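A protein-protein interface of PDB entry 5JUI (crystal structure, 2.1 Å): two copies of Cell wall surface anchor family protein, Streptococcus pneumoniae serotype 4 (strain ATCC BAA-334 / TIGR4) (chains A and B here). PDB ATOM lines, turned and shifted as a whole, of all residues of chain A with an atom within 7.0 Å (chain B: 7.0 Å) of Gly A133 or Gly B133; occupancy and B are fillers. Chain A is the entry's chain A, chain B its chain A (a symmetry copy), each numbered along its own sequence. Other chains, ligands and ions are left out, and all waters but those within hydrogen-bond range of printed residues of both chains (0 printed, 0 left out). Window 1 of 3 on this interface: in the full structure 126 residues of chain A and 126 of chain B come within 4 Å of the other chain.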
ATOM      1  N   THR A  98      17.703 -18.295 -11.190  1.00  0.00           N
ATOM      2  CA  THR A  98      16.316 -18.682 -10.938  1.00  0.00           C
ATOM      3  C   THR A  98      15.667 -19.105 -12.247  1.00  0.00           C
ATOM      4  O   THR A  98      15.783 -18.409 -13.252  1.00  0.00           O
ATOM      5  CB  THR A  98      15.494 -17.537 -10.308  1.00  0.00           C
ATOM      6  OG1 THR A  98      15.263 -16.513 -11.283  1.00  0.00           O
ATOM      7  CG2 THR A  98      16.235 -16.947  -9.117  1.00  0.00           C
ATOM      8  N   LEU A  99      14.976 -20.238 -12.235  1.00  0.00           N
ATOM      9  CA  LEU A  99      14.455 -20.810 -13.469  1.00  0.00           C
ATOM     10  C   LEU A  99      12.930 -20.856 -13.497  1.00  0.00           C
ATOM     11  O   LEU A  99      12.289 -21.123 -12.480  1.00  0.00           O
ATOM     12  CB  LEU A  99      15.023 -22.219 -13.661  1.00  0.00           C
ATOM     13  CG  LEU A  99      16.549 -22.292 -13.786  1.00  0.00           C
ATOM     14  CD1 LEU A  99      17.026 -23.727 -13.920  1.00  0.00           C
ATOM     15  CD2 LEU A  99      17.007 -21.479 -14.991  1.00  0.00           C
ATOM     16  N   GLY A 100      12.358 -20.613 -14.674  1.00  0.00           N
ATOM     17  CA  GLY A 100      10.916 -20.640 -14.850  1.00  0.00           C
ATOM     18  C   GLY A 100      10.361 -22.048 -14.792  1.00  0.00           C
ATOM     19  O   GLY A 100      11.123 -23.011 -14.740  1.00  0.00           O
ATOM     20  N   SER A 101       9.038 -22.170 -14.850  1.00  0.00           N
ATOM     21  CA  SER A 101       8.375 -23.441 -14.572  1.00  0.00           C
ATOM     22  C   SER A 101       8.577 -24.506 -15.648  1.00  0.00           C
ATOM     23  O   SER A 101       8.458 -25.698 -15.366  1.00  0.00           O
ATOM     24  CB  SER A 101       6.878 -23.226 -14.322  1.00  0.00           C
ATOM     25  OG  SER A 101       6.251 -22.627 -15.440  1.00  0.00           O
ATOM     26  N   THR A 130      22.857 -26.760  -6.375  1.00  0.00           N
ATOM     27  CA  THR A 130      21.931 -27.095  -5.293  1.00  0.00           C
ATOM     28  C   THR A 130      20.773 -26.098  -5.295  1.00  0.00           C
ATOM     29  O   THR A 130      20.983 -24.895  -5.467  1.00  0.00           O
ATOM     30  CB  THR A 130      22.626 -27.094  -3.911  1.00  0.00           C
ATOM     31  OG1 THR A 130      23.349 -25.869  -3.728  1.00  0.00           O
ATOM     32  CG2 THR A 130      23.596 -28.266  -3.804  1.00  0.00           C
ATOM     33  N   THR A 131      19.550 -26.598  -5.150  1.00  0.00           N
ATOM     34  CA  THR A 131      18.383 -25.726  -5.232  1.00  0.00           C
ATOM     35  C   THR A 131      18.096 -25.056  -3.895  1.00  0.00           C
ATOM     36  O   THR A 131      18.329 -25.630  -2.831  1.00  0.00           O
ATOM     37  CB  THR A 131      17.126 -26.487  -5.709  1.00  0.00           C
ATOM     38  OG1 THR A 131      16.039 -25.563  -5.866  1.00  0.00           O
ATOM     39  CG2 THR A 131      16.732 -27.581  -4.721  1.00  0.00           C
ATOM     40  N   GLN A 132      17.586 -23.833  -3.960  1.00  0.00           N
ATOM     41  CA  GLN A 132      17.102 -23.138  -2.779  1.00  0.00           C
ATOM     42  C   GLN A 132      15.591 -23.288  -2.680  1.00  0.00           C
ATOM     43  O   GLN A 132      14.960 -22.754  -1.772  1.00  0.00           O
ATOM     44  CB  GLN A 132      17.502 -21.671  -2.847  1.00  0.00           C
ATOM     45  CG  GLN A 132      18.900 -21.438  -2.319  1.00  0.00           C
ATOM     46  CD  GLN A 132      19.949 -21.781  -3.358  1.00  0.00           C
ATOM     47  OE1 GLN A 132      19.920 -21.262  -4.473  1.00  0.00           O
ATOM     48  NE2 GLN A 132      20.864 -22.682  -3.009  1.00  0.00           N
ATOM     49  N   GLY A 133      15.020 -24.004  -3.643  1.00  0.00           N
ATOM     50  CA  GLY A 133      13.596 -24.280  -3.661  1.00  0.00           C
ATOM     51  C   GLY A 133      12.830 -23.419  -4.648  1.00  0.00           C
ATOM     52  O   GLY A 133      13.390 -22.513  -5.265  1.00  0.00           O
ATOM     53  N   SER A 134      11.547 -23.722  -4.817  1.00  0.00           N
ATOM     54  CA  SER A 134      10.686 -22.952  -5.709  1.00  0.00           C
ATOM     55  C   SER A 134       9.829 -22.001  -4.886  1.00  0.00           C
ATOM     56  O   SER A 134       9.166 -22.421  -3.935  1.00  0.00           O
ATOM     57  CB  SER A 134       9.790 -23.880  -6.526  1.00  0.00           C
ATOM     58  OG  SER A 134      10.530 -24.949  -7.084  1.00  0.00           O
ATOM     59  N   GLY A 135       9.825 -20.724  -5.254  1.00  0.00           N
ATOM     60  CA  GLY A 135       9.046 -19.739  -4.524  1.00  0.00           C
ATOM     61  C   GLY A 135       7.655 -19.530  -5.091  1.00  0.00           C
ATOM     62  O   GLY A 135       7.448 -19.586  -6.305  1.00  0.00           O
ATOM     63  N   TYR A 136       6.694 -19.274  -4.210  1.00  0.00           N
ATOM     64  CA  TYR A 136       5.312 -19.134  -4.645  1.00  0.00           C
ATOM     65  C   TYR A 136       4.591 -17.996  -3.941  1.00  0.00           C
ATOM     66  O   TYR A 136       4.925 -17.623  -2.813  1.00  0.00           O
ATOM     67  CB  TYR A 136       4.527 -20.428  -4.402  1.00  0.00           C
ATOM     68  CG  TYR A 136       4.943 -21.602  -5.256  1.00  0.00           C
ATOM     69  CD1 TYR A 136       4.357 -21.829  -6.494  1.00  0.00           C
ATOM     70  CD2 TYR A 136       5.908 -22.493  -4.815  1.00  0.00           C
ATOM     71  CE1 TYR A 136       4.733 -22.909  -7.272  1.00  0.00           C
ATOM     72  CE2 TYR A 136       6.287 -23.572  -5.586  1.00  0.00           C
ATOM     73  CZ  TYR A 136       5.699 -23.774  -6.811  1.00  0.00           C
ATOM     74  OH  TYR A 136       6.077 -24.851  -7.574  1.00  0.00           O
ATOM     75  N   THR B  98       8.132 -21.259  -0.058  1.00  0.00           N
ATOM     76  CA  THR B  98       9.188 -21.873  -0.860  1.00  0.00           C
ATOM     77  C   THR B  98       9.202 -23.373  -0.610  1.00  0.00           C
ATOM     78  O   THR B  98       9.171 -23.812   0.537  1.00  0.00           O
ATOM     79  CB  THR B  98      10.581 -21.289  -0.539  1.00  0.00           C
ATOM     80  OG1 THR B  98      11.005 -21.731   0.756  1.00  0.00           O
ATOM     81  CG2 THR B  98      10.538 -19.768  -0.569  1.00  0.00           C
ATOM     82  N   LEU B  99       9.259 -24.159  -1.678  1.00  0.00           N
ATOM     83  CA  LEU B  99       9.115 -25.603  -1.553  1.00  0.00           C
ATOM     84  C   LEU B  99      10.375 -26.357  -1.965  1.00  0.00           C
ATOM     85  O   LEU B  99      11.054 -25.976  -2.919  1.00  0.00           O
ATOM     86  CB  LEU B  99       7.926 -26.073  -2.395  1.00  0.00           C
ATOM     87  CG  LEU B  99       6.570 -25.488  -1.988  1.00  0.00           C
ATOM     88  CD1 LEU B  99       5.460 -25.967  -2.907  1.00  0.00           C
ATOM     89  CD2 LEU B  99       6.252 -25.874  -0.548  1.00  0.00           C
ATOM     90  N   GLY B 100      10.669 -27.441  -1.251  1.00  0.00           N
ATOM     91  CA  GLY B 100      11.831 -28.264  -1.543  1.00  0.00           C
ATOM     92  C   GLY B 100      11.656 -29.065  -2.816  1.00  0.00           C
ATOM     93  O   GLY B 100      10.574 -29.069  -3.401  1.00  0.00           O
ATOM     94  N   SER B 101      12.703 -29.781  -3.219  1.00  0.00           N
ATOM     95  CA  SER B 101      12.740 -30.404  -4.539  1.00  0.00           C
ATOM     96  C   SER B 101      11.794 -31.591  -4.703  1.00  0.00           C
ATOM     97  O   SER B 101      11.410 -31.924  -5.823  1.00  0.00           O
ATOM     98  CB  SER B 101      14.170 -30.819  -4.899  1.00  0.00           C
ATOM     99  OG  SER B 101      14.693 -31.734  -3.955  1.00  0.00           O
ATOM    100  N   THR B 130       1.053 -18.620  -8.079  1.00  0.00           N
ATOM    101  CA  THR B 130       1.959 -18.350  -9.197  1.00  0.00           C
ATOM    102  C   THR B 130       3.403 -18.479  -8.716  1.00  0.00           C
ATOM    103  O   THR B 130       3.744 -18.014  -7.627  1.00  0.00           O
ATOM    104  CB  THR B 130       1.726 -16.947  -9.806  1.00  0.00           C
ATOM    105  OG1 THR B 130       1.736 -15.956  -8.769  1.00  0.00           O
ATOM    106  CG2 THR B 130       0.386 -16.898 -10.531  1.00  0.00           C
ATOM    107  N   THR B 131       4.241 -19.146  -9.503  1.00  0.00           N
ATOM    108  CA  THR B 131       5.614 -19.392  -9.078  1.00  0.00           C
ATOM    109  C   THR B 131       6.515 -18.205  -9.393  1.00  0.00           C
ATOM    110  O   THR B 131       6.323 -17.506 -10.388  1.00  0.00           O
ATOM    111  CB  THR B 131       6.198 -20.669  -9.722  1.00  0.00           C
ATOM    112  OG1 THR B 131       7.509 -20.916  -9.192  1.00  0.00           O
ATOM    113  CG2 THR B 131       6.273 -20.539 -11.240  1.00  0.00           C
ATOM    114  N   GLN B 132       7.501 -17.985  -8.534  1.00  0.00           N
ATOM    115  CA  GLN B 132       8.540 -17.002  -8.791  1.00  0.00           C
ATOM    116  C   GLN B 132       9.772 -17.694  -9.353  1.00  0.00           C
ATOM    117  O   GLN B 132      10.790 -17.059  -9.619  1.00  0.00           O
ATOM    118  CB  GLN B 132       8.871 -16.256  -7.506  1.00  0.00           C
ATOM    119  CG  GLN B 132       7.933 -15.094  -7.266  1.00  0.00           C
ATOM    120  CD  GLN B 132       6.619 -15.556  -6.670  1.00  0.00           C
ATOM    121  OE1 GLN B 132       6.599 -16.222  -5.636  1.00  0.00           O
ATOM    122  NE2 GLN B 132       5.514 -15.231  -7.336  1.00  0.00           N
ATOM    123  N   GLY B 133       9.671 -19.010  -9.509  1.00  0.00           N
ATOM    124  CA  GLY B 133      10.742 -19.805 -10.081  1.00  0.00           C
ATOM    125  C   GLY B 133      11.539 -20.574  -9.042  1.00  0.00           C
ATOM    126  O   GLY B 133      11.330 -20.416  -7.840  1.00  0.00           O
ATOM    127  N   SER B 134      12.438 -21.433  -9.512  1.00  0.00           N
ATOM    128  CA  SER B 134      13.297 -22.210  -8.624  1.00  0.00           C
ATOM    129  C   SER B 134      14.679 -21.573  -8.574  1.00  0.00           C
ATOM    130  O   SER B 134      15.287 -21.318  -9.615  1.00  0.00           O
ATOM    131  CB  SER B 134      13.410 -23.653  -9.112  1.00  0.00           C
ATOM    132  OG  SER B 134      12.141 -24.186  -9.436  1.00  0.00           O
ATOM    133  N   GLY B 135      15.184 -21.330  -7.370  1.00  0.00           N
ATOM    134  CA  GLY B 135      16.491 -20.715  -7.219  1.00  0.00           C
ATOM    135  C   GLY B 135      17.620 -21.721  -7.091  1.00  0.00           C
ATOM    136  O   GLY B 135      17.456 -22.788  -6.494  1.00  0.00           O
ATOM    137  N   TYR B 136      18.778 -21.378  -7.642  1.00  0.00           N
ATOM    138  CA  TYR B 136      19.901 -22.304  -7.640  1.00  0.00           C
ATOM    139  C   TYR B 136      21.224 -21.619  -7.340  1.00  0.00           C
ATOM    140  O   TYR B 136      21.406 -20.428  -7.608  1.00  0.00           O
ATOM    141  CB  TYR B 136      20.021 -23.021  -8.989  1.00  0.00           C
ATOM    142  CG  TYR B 136      18.901 -23.982  -9.310  1.00  0.00           C
ATOM    143  CD1 TYR B 136      18.971 -25.315  -8.930  1.00  0.00           C
ATOM    144  CD2 TYR B 136      17.781 -23.558 -10.008  1.00  0.00           C
ATOM    145  CE1 TYR B 136      17.948 -26.196  -9.231  1.00  0.00           C
ATOM    146  CE2 TYR B 136      16.758 -24.431 -10.310  1.00  0.00           C
ATOM    147  CZ  TYR B 136      16.845 -25.745  -9.920  1.00  0.00           C
ATOM    148  OH  TYR B 136      15.825 -26.612 -10.227  1.00  0.00           O
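The backbone carbonyl oxygen (O) of Ser B134 sits at hydrogen-bond distance from the backbone NH (N) of Leu A99.
OG1 of Thr A131 sits at hydrogen-bond distance from O of Gly B135 (3.2 Å).
The backbone carbonyl oxygen of Gly B135 sits at hydrogen-bond distance from the backbone NH of Gln A132.
OE1 of Gln A132 lies close to N of Tyr B136.
N of Gly B135 lies within hydrogen-bond range of O of Gly A133 (3.0 Å).
O of Ser A134 lies within hydrogen-bond range of N of Leu B99 (2.9 Å).
OG of Ser A134 sits at hydrogen-bond distance from OG of Ser B134, at 3.0 Å.
The side-chain hydroxyl (OG1) of Thr B131 lies within hydrogen-bond range of the backbone carbonyl oxygen (O) of Gly A135.
The backbone NH (N) of Gln B132 is in hydrogen-bond range of the backbone carbonyl oxygen (O) of Gly A135.
The backbone NH of Gly A135 lies within hydrogen-bond range of the backbone carbonyl oxygen of Gly B133, at 3.0 Å.
N of Tyr A136 lies close to OE1 of Gln B132.
O of Thr A130 is in hydrogen-bond range of NE2 of Gln A132.
N of Gly A133 lies within hydrogen-bond range of OG1 of Thr A131 (2.9 Å).
The side-chain amide nitrogen of Gln B132 sits at hydrogen-bond distance from the backbone carbonyl oxygen of Thr B130 (3.3 Å).
N of Gly B133 sits at hydrogen-bond distance from OG1 of Thr B131 (2.9 Å).
Ser B134 touches Thr A98 (O to CA, 3.1 Å).
Gly B133 touches Leu A99 (CA to O, 3.1 Å).
Tyr B136 touches Leu A99 (CE2 to CD1, 3.7 Å).
Thr A130 touches Tyr B136 (O to CA, 3.6 Å).
Thr A131 touches Tyr B136 (CB to CE1, 3.6 Å).
CA of Gly A133 touches O of Leu B99, 3.1 Å away.
CA of Ser B134 touches O of Gly A133, 3.4 Å away.
Ser A134 touches Gly B133 (CA to O, 3.4 Å).
Leu B99 touches Tyr A136.
Thr B130 touches Tyr A136 (O to CA, 3.6 Å).
Ser A101 touches none of the printed residues of chain B.
Gly A133 touches four residues of chain B.
Printed residues of chain B within 4 Å of Tyr A136: Leu B99 (3.7 Å), Thr B130 (3.6 Å), Thr B131 (3.6 Å) and Gln B132 (3.2 Å).
Of the printed residues of chain A, Leu B99 touches Gly A133 (3.1 Å), Ser A134 (2.9 Å) and Tyr A136 (3.7 Å).
Ser B101 touches none of the printed residues of chain A.
Gly B133 touches four residues of chain A.
Printed residues of chain A within 4 Å of Ser B134: Thr A98 (3.1 Å), Leu A99 (2.9 Å), Gly A133 (3.4 Å) and Ser A134 (3.0 Å).
The nearest residue of chain A that does not touch Gly B133 is Gly A100 (4.8 Å).
The nearest printed residue of chain A that does not touch Gln B132 is Thr A98 (4.8 Å).
Printed residues of chain B that touch a printed residue of chain A: Thr B98, Leu B99, Thr B130, Thr B131, Gln B132, Gly B133, Ser B134, Gly B135 and Tyr B136.
Hydrophobic or aromatic side chains of chain B within 4 Å of the printed part of chain A: Leu B99 and Tyr B136.
Among the printed residues, no Asp or Glu carboxylate lies within 4 Å of a Lys or Arg side-chain nitrogen of the other chain.
Thr A98 touches Ser B134, and with the chains exchanged Ser A134 touches Thr B98.
Leu A99 touches Tyr B136, and with the chains exchanged Tyr A136 touches Leu B99.
Gly B133 touches its own counterpart, Gly A133.
Gly A133 touches Gly B135, and with the chains exchanged Gly A135 touches Gly B133.
11 positions are printed for both chains.
Of the 24 pairs that touch across the chains among the printed residues, 24 have their exchanged pair printed and touching as well.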
